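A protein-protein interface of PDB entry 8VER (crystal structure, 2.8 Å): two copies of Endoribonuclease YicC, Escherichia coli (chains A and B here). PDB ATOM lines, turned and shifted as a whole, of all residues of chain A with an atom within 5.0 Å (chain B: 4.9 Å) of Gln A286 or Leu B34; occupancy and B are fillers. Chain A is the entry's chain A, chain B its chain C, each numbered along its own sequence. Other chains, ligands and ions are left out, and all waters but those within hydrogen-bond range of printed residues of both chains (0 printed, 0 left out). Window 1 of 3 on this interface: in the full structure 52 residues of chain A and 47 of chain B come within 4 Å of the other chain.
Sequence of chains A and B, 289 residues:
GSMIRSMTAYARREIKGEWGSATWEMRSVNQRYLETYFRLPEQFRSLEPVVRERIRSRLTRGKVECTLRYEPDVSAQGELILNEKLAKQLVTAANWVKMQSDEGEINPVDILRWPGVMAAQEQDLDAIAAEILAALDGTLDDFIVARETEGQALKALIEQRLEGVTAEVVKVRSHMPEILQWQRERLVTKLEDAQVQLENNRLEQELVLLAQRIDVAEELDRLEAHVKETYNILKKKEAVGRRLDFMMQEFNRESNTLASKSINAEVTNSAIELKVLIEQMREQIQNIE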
ATOM      1  N   MET A   7       1.562  19.471  23.392  1.00  0.00           N
ATOM      2  CA  MET A   7       2.039  20.357  24.447  1.00  0.00           C
ATOM      3  C   MET A   7       0.908  21.147  25.095  1.00  0.00           C
ATOM      4  O   MET A   7       1.017  21.522  26.268  1.00  0.00           O
ATOM      5  CB  MET A   7       3.099  21.312  23.894  1.00  0.00           C
ATOM      6  CG  MET A   7       4.470  20.675  23.736  1.00  0.00           C
ATOM      7  SD  MET A   7       5.732  21.793  23.097  1.00  0.00           S
ATOM      8  CE  MET A   7       5.126  22.075  21.438  1.00  0.00           C
ATOM      9  N   ASN A  30       2.388  25.662  23.831  1.00  0.00           N
ATOM     10  CA  ASN A  30       3.605  25.252  23.148  1.00  0.00           C
ATOM     11  C   ASN A  30       4.787  26.126  23.551  1.00  0.00           C
ATOM     12  O   ASN A  30       4.642  27.315  23.853  1.00  0.00           O
ATOM     13  CB  ASN A  30       3.403  25.305  21.635  1.00  0.00           C
ATOM     14  CG  ASN A  30       2.334  24.344  21.163  1.00  0.00           C
ATOM     15  OD1 ASN A  30       1.687  23.674  21.969  1.00  0.00           O
ATOM     16  ND2 ASN A  30       2.136  24.278  19.853  1.00  0.00           N
ATOM     17  N   ARG A  61       8.751  19.111  27.639  1.00  0.00           N
ATOM     18  CA  ARG A  61       8.844  20.505  27.228  1.00  0.00           C
ATOM     19  C   ARG A  61       7.445  21.101  27.132  1.00  0.00           C
ATOM     20  O   ARG A  61       6.438  20.393  27.191  1.00  0.00           O
ATOM     21  CB  ARG A  61       9.599  20.650  25.904  1.00  0.00           C
ATOM     22  CG  ARG A  61       8.871  20.106  24.693  1.00  0.00           C
ATOM     23  CD  ARG A  61       9.804  20.053  23.499  1.00  0.00           C
ATOM     24  NE  ARG A  61       9.089  19.839  22.249  1.00  0.00           N
ATOM     25  CZ  ARG A  61       8.776  20.801  21.393  1.00  0.00           C
ATOM     26  NH1 ARG A  61       9.109  22.061  21.619  1.00  0.00           N
ATOM     27  NH2 ARG A  61       8.117  20.491  20.280  1.00  0.00           N
ATOM     28  N   ARG A 282       3.801  20.029   9.258  1.00  0.00           N
ATOM     29  CA  ARG A 282       4.528  20.930  10.148  1.00  0.00           C
ATOM     30  C   ARG A 282       3.585  21.640  11.112  1.00  0.00           C
ATOM     31  O   ARG A 282       3.939  21.879  12.273  1.00  0.00           O
ATOM     32  CB  ARG A 282       5.319  21.952   9.332  1.00  0.00           C
ATOM     33  CG  ARG A 282       6.652  21.448   8.813  1.00  0.00           C
ATOM     34  CD  ARG A 282       7.286  22.475   7.891  1.00  0.00           C
ATOM     35  NE  ARG A 282       8.690  22.188   7.624  1.00  0.00           N
ATOM     36  CZ  ARG A 282       9.419  22.820   6.715  1.00  0.00           C
ATOM     37  NH1 ARG A 282       8.901  23.769   5.953  1.00  0.00           N
ATOM     38  NH2 ARG A 282      10.699  22.490   6.566  1.00  0.00           N
ATOM     39  N   GLU A 283       2.383  21.991  10.648  1.00  0.00           N
ATOM     40  CA  GLU A 283       1.425  22.664  11.521  1.00  0.00           C
ATOM     41  C   GLU A 283       0.988  21.751  12.659  1.00  0.00           C
ATOM     42  O   GLU A 283       0.797  22.207  13.793  1.00  0.00           O
ATOM     43  CB  GLU A 283       0.218  23.140  10.710  1.00  0.00           C
ATOM     44  CG  GLU A 283      -0.551  24.297  11.342  1.00  0.00           C
ATOM     45  CD  GLU A 283      -1.422  23.867  12.507  1.00  0.00           C
ATOM     46  OE1 GLU A 283      -2.015  22.770  12.433  1.00  0.00           O
ATOM     47  OE2 GLU A 283      -1.509  24.621  13.500  1.00  0.00           O
ATOM     48  N   GLN A 284       0.820  20.457  12.378  1.00  0.00           N
ATOM     49  CA  GLN A 284       0.504  19.512  13.444  1.00  0.00           C
ATOM     50  C   GLN A 284       1.718  19.237  14.321  1.00  0.00           C
ATOM     51  O   GLN A 284       1.573  19.017  15.528  1.00  0.00           O
ATOM     52  CB  GLN A 284      -0.023  18.204  12.851  1.00  0.00           C
ATOM     53  CG  GLN A 284      -0.897  18.373  11.617  1.00  0.00           C
ATOM     54  CD  GLN A 284      -2.140  19.197  11.882  1.00  0.00           C
ATOM     55  OE1 GLN A 284      -2.646  19.239  13.004  1.00  0.00           O
ATOM     56  NE2 GLN A 284      -2.638  19.861  10.846  1.00  0.00           N
ATOM     57  N   ILE A 285       2.918  19.253  13.736  1.00  0.00           N
ATOM     58  CA  ILE A 285       4.120  18.911  14.486  1.00  0.00           C
ATOM     59  C   ILE A 285       4.476  20.004  15.485  1.00  0.00           C
ATOM     60  O   ILE A 285       5.003  19.717  16.569  1.00  0.00           O
ATOM     61  CB  ILE A 285       5.273  18.615  13.506  1.00  0.00           C
ATOM     62  CG1 ILE A 285       5.090  17.225  12.894  1.00  0.00           C
ATOM     63  CG2 ILE A 285       6.629  18.721  14.189  1.00  0.00           C
ATOM     64  CD1 ILE A 285       6.073  16.897  11.804  1.00  0.00           C
ATOM     65  N   GLN A 286       4.175  21.267  15.165  1.00  0.00           N
ATOM     66  CA  GLN A 286       4.498  22.356  16.082  1.00  0.00           C
ATOM     67  C   GLN A 286       3.768  22.219  17.410  1.00  0.00           C
ATOM     68  O   GLN A 286       4.187  22.824  18.402  1.00  0.00           O
ATOM     69  CB  GLN A 286       4.168  23.709  15.447  1.00  0.00           C
ATOM     70  CG  GLN A 286       2.702  24.098  15.527  1.00  0.00           C
ATOM     71  CD  GLN A 286       2.467  25.551  15.168  1.00  0.00           C
ATOM     72  OE1 GLN A 286       3.377  26.245  14.711  1.00  0.00           O
ATOM     73  NE2 GLN A 286       1.244  26.023  15.378  1.00  0.00           N
ATOM     74  N   ASN A 287       2.691  21.437  17.449  1.00  0.00           N
ATOM     75  CA  ASN A 287       1.962  21.177  18.680  1.00  0.00           C
ATOM     76  C   ASN A 287       2.424  19.910  19.385  1.00  0.00           C
ATOM     77  O   ASN A 287       1.990  19.655  20.513  1.00  0.00           O
ATOM     78  CB  ASN A 287       0.460  21.081  18.391  1.00  0.00           C
ATOM     79  CG  ASN A 287      -0.060  22.275  17.614  1.00  0.00           C
ATOM     80  OD1 ASN A 287      -0.138  23.386  18.138  1.00  0.00           O
ATOM     81  ND2 ASN A 287      -0.428  22.050  16.357  1.00  0.00           N
ATOM     82  N   ILE A 288       3.289  19.119  18.755  1.00  0.00           N
ATOM     83  CA  ILE A 288       3.769  17.876  19.345  1.00  0.00           C
ATOM     84  C   ILE A 288       4.929  18.173  20.284  1.00  0.00           C
ATOM     85  O   ILE A 288       5.820  18.972  19.968  1.00  0.00           O
ATOM     86  CB  ILE A 288       4.180  16.881  18.246  1.00  0.00           C
ATOM     87  CG1 ILE A 288       2.958  16.443  17.440  1.00  0.00           C
ATOM     88  CG2 ILE A 288       4.871  15.670  18.845  1.00  0.00           C
ATOM     89  CD1 ILE A 288       3.277  15.430  16.374  1.00  0.00           C
ATOM     90  N   ARG B  32       2.201  31.879   9.389  1.00  0.00           N
ATOM     91  CA  ARG B  32       2.516  30.692   8.602  1.00  0.00           C
ATOM     92  C   ARG B  32       1.694  29.496   9.066  1.00  0.00           C
ATOM     93  O   ARG B  32       1.218  28.704   8.244  1.00  0.00           O
ATOM     94  CB  ARG B  32       4.013  30.388   8.682  1.00  0.00           C
ATOM     95  CG  ARG B  32       4.489  29.318   7.713  1.00  0.00           C
ATOM     96  CD  ARG B  32       5.961  28.994   7.921  1.00  0.00           C
ATOM     97  NE  ARG B  32       6.476  28.122   6.873  1.00  0.00           N
ATOM     98  CZ  ARG B  32       7.699  27.607   6.859  1.00  0.00           C
ATOM     99  NH1 ARG B  32       8.558  27.839   7.839  1.00  0.00           N
ATOM    100  NH2 ARG B  32       8.068  26.837   5.839  1.00  0.00           N
ATOM    101  N   TYR B  33       1.509  29.350  10.378  1.00  0.00           N
ATOM    102  CA  TYR B  33       0.670  28.281  10.905  1.00  0.00           C
ATOM    103  C   TYR B  33      -0.443  28.869  11.764  1.00  0.00           C
ATOM    104  O   TYR B  33      -0.740  30.064  11.663  1.00  0.00           O
ATOM    105  CB  TYR B  33       1.511  27.278  11.702  1.00  0.00           C
ATOM    106  CG  TYR B  33       2.714  26.757  10.943  1.00  0.00           C
ATOM    107  CD1 TYR B  33       2.571  25.806   9.940  1.00  0.00           C
ATOM    108  CD2 TYR B  33       3.990  27.222  11.229  1.00  0.00           C
ATOM    109  CE1 TYR B  33       3.669  25.333   9.243  1.00  0.00           C
ATOM    110  CE2 TYR B  33       5.091  26.755  10.539  1.00  0.00           C
ATOM    111  CZ  TYR B  33       4.925  25.812   9.549  1.00  0.00           C
ATOM    112  OH  TYR B  33       6.022  25.350   8.863  1.00  0.00           O
ATOM    113  N   LEU B  34      -1.069  28.052  12.606  1.00  0.00           N
ATOM    114  CA  LEU B  34      -2.167  28.503  13.451  1.00  0.00           C
ATOM    115  C   LEU B  34      -1.667  28.695  14.878  1.00  0.00           C
ATOM    116  O   LEU B  34      -1.130  27.761  15.485  1.00  0.00           O
ATOM    117  CB  LEU B  34      -3.332  27.514  13.422  1.00  0.00           C
ATOM    118  CG  LEU B  34      -4.575  27.956  14.202  1.00  0.00           C
ATOM    119  CD1 LEU B  34      -5.190  29.218  13.611  1.00  0.00           C
ATOM    120  CD2 LEU B  34      -5.603  26.845  14.258  1.00  0.00           C
ATOM    121  N   GLU B  35      -1.842  29.906  15.405  1.00  0.00           N
ATOM    122  CA  GLU B  35      -1.504  30.228  16.786  1.00  0.00           C
ATOM    123  C   GLU B  35      -2.690  30.943  17.414  1.00  0.00           C
ATOM    124  O   GLU B  35      -3.090  32.013  16.948  1.00  0.00           O
ATOM    125  CB  GLU B  35      -0.244  31.095  16.865  1.00  0.00           C
ATOM    126  CG  GLU B  35       1.034  30.372  16.461  1.00  0.00           C
ATOM    127  CD  GLU B  35       2.273  31.208  16.713  1.00  0.00           C
ATOM    128  OE1 GLU B  35       2.125  32.407  17.026  1.00  0.00           O
ATOM    129  OE2 GLU B  35       3.395  30.666  16.604  1.00  0.00           O
ATOM    130  N   THR B  36      -3.254  30.348  18.461  1.00  0.00           N
ATOM    131  CA  THR B  36      -4.430  30.879  19.135  1.00  0.00           C
ATOM    132  C   THR B  36      -4.065  31.318  20.547  1.00  0.00           C
ATOM    133  O   THR B  36      -3.361  30.603  21.267  1.00  0.00           O
ATOM    134  CB  THR B  36      -5.551  29.837  19.188  1.00  0.00           C
ATOM    135  OG1 THR B  36      -5.099  28.684  19.908  1.00  0.00           O
ATOM    136  CG2 THR B  36      -5.954  29.417  17.784  1.00  0.00           C
ATOM    137  N   ARG B  56     -10.084  25.942  16.742  1.00  0.00           N
ATOM    138  CA  ARG B  56      -9.207  25.095  15.942  1.00  0.00           C
ATOM    139  C   ARG B  56      -9.962  24.402  14.816  1.00  0.00           C
ATOM    140  O   ARG B  56      -9.393  24.154  13.746  1.00  0.00           O
ATOM    141  CB  ARG B  56      -8.534  24.059  16.847  1.00  0.00           C
ATOM    142  CG  ARG B  56      -7.527  23.152  16.157  1.00  0.00           C
ATOM    143  CD  ARG B  56      -6.151  23.790  16.099  1.00  0.00           C
ATOM    144  NE  ARG B  56      -5.720  24.270  17.408  1.00  0.00           N
ATOM    145  CZ  ARG B  56      -4.523  24.779  17.663  1.00  0.00           C
ATOM    146  NH1 ARG B  56      -3.597  24.873  16.722  1.00  0.00           N
ATOM    147  NH2 ARG B  56      -4.247  25.204  18.892  1.00  0.00           N
ATOM    148  N   LEU B  59     -10.707  27.024  11.851  1.00  0.00           N
ATOM    149  CA  LEU B  59      -9.562  27.786  11.373  1.00  0.00           C
ATOM    150  C   LEU B  59      -8.376  26.859  11.156  1.00  0.00           C
ATOM    151  O   LEU B  59      -8.112  25.971  11.973  1.00  0.00           O
ATOM    152  CB  LEU B  59      -9.180  28.892  12.361  1.00  0.00           C
ATOM    153  CG  LEU B  59     -10.290  29.884  12.701  1.00  0.00           C
ATOM    154  CD1 LEU B  59      -9.781  30.938  13.667  1.00  0.00           C
ATOM    155  CD2 LEU B  59     -10.830  30.527  11.435  1.00  0.00           C
ATOM    156  N   THR B  60      -7.660  27.072  10.055  1.00  0.00           N
ATOM    157  CA  THR B  60      -6.479  26.285   9.720  1.00  0.00           C
ATOM    158  C   THR B  60      -5.173  27.030   9.942  1.00  0.00           C
ATOM    159  O   THR B  60      -4.211  26.441  10.437  1.00  0.00           O
ATOM    160  CB  THR B  60      -6.544  25.825   8.259  1.00  0.00           C
ATOM    161  OG1 THR B  60      -6.246  26.929   7.396  1.00  0.00           O
ATOM    162  CG2 THR B  60      -7.933  25.298   7.926  1.00  0.00           C
ATOM    163  N   ARG B  61      -5.104  28.310   9.579  1.00  0.00           N
ATOM    164  CA  ARG B  61      -3.898  29.104   9.770  1.00  0.00           C
ATOM    165  C   ARG B  61      -4.285  30.493  10.248  1.00  0.00           C
ATOM    166  O   ARG B  61      -5.424  30.938  10.090  1.00  0.00           O
ATOM    167  CB  ARG B  61      -3.064  29.197   8.482  1.00  0.00           C
ATOM    168  CG  ARG B  61      -2.737  27.857   7.838  1.00  0.00           C
ATOM    169  CD  ARG B  61      -1.676  27.977   6.748  1.00  0.00           C
ATOM    170  NE  ARG B  61      -2.019  28.964   5.730  1.00  0.00           N
ATOM    171  CZ  ARG B  61      -1.383  30.116   5.561  1.00  0.00           C
ATOM    172  NH1 ARG B  61      -0.350  30.452   6.316  1.00  0.00           N
ATOM    173  NH2 ARG B  61      -1.789  30.947   4.606  1.00  0.00           N
ATOM    174  N   GLY B  62      -3.315  31.187  10.844  1.00  0.00           N
ATOM    175  CA  GLY B  62      -3.505  32.526  11.332  1.00  0.00           C
ATOM    176  C   GLY B  62      -3.181  32.656  12.815  1.00  0.00           C
ATOM    177  O   GLY B  62      -3.018  31.666  13.531  1.00  0.00           O
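The guanidinium group (NH2) of Arg B32 sits close to the guanidinium group (NH1) of Arg A282 (3.2 Å). The side-chain carboxylate of Glu A283 lies within salt-bridge range of the guanidinium group of Arg B56 (3.8 Å). The side-chain amide nitrogen (NE2) of Gln A286 is in hydrogen-bond range of the backbone carbonyl oxygen (O) of Leu B34 (2.9 Å).
The guanidinium group of Arg B32 is in hydrogen-bond range of the side-chain hydroxyl of Tyr B33 (3.4 Å). NH1 of Arg B61 lies within hydrogen-bond range of O of Arg B32 (3.0 Å). The side-chain amide nitrogen (ND2) of Asn A287 lies within hydrogen-bond range of the backbone carbonyl oxygen (O) of Glu A283 (2.8 Å). NE2 of Gln A284 is in hydrogen-bond range of OE1 of Glu A283 (3.4 Å). ND2 of Asn A30 lies within hydrogen-bond range of O of Gln A286, at 2.9 Å. The backbone NH (N) of Gly B62 is in hydrogen-bond range of the backbone carbonyl oxygen (O) of Tyr B33 (2.9 Å).
Among the printed residues, pairs that only touch across the chains: Arg A282 with Tyr B33, Glu A283 with Tyr B33, Glu A283 with Leu B34 and Gln A286 with Tyr B33.
Of the printed residues of chain B, Arg A282 touches Arg B32 and Tyr B33. Gln A286 touches two residues of chain B. Ile A288 touches none of the printed residues of chain B. Of the printed residues of chain A, Tyr B33 touches Arg A282, Glu A283 and Gln A286. Leu B34 touches just these residues of chain A: Glu A283 and Gln A286. Arg B61 touches none of the printed residues of chain A. The nearest residue of chain B that does not touch Gln A286 is Glu B35 (4.5 Å).
Along chain A the printed residues that touch a printed residue of chain B span positions 282 to 286. Of the 10 printed residues of chain B, 4 touch a printed residue of chain A. Printed residues of chain B that touch a printed residue of chain A: Arg B32, Tyr B33, Leu B34 and Arg B56. Among the printed residues, Asp or Glu carboxylates within 4 Å of a Lys or Arg side-chain nitrogen of the other chain: Glu A283 with Arg B56 (3.8 Å).
1 position is printed for both chains. Of the 7 pairs that touch across the chains among the printed residues, none has its exchanged pair printed and touching as well.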
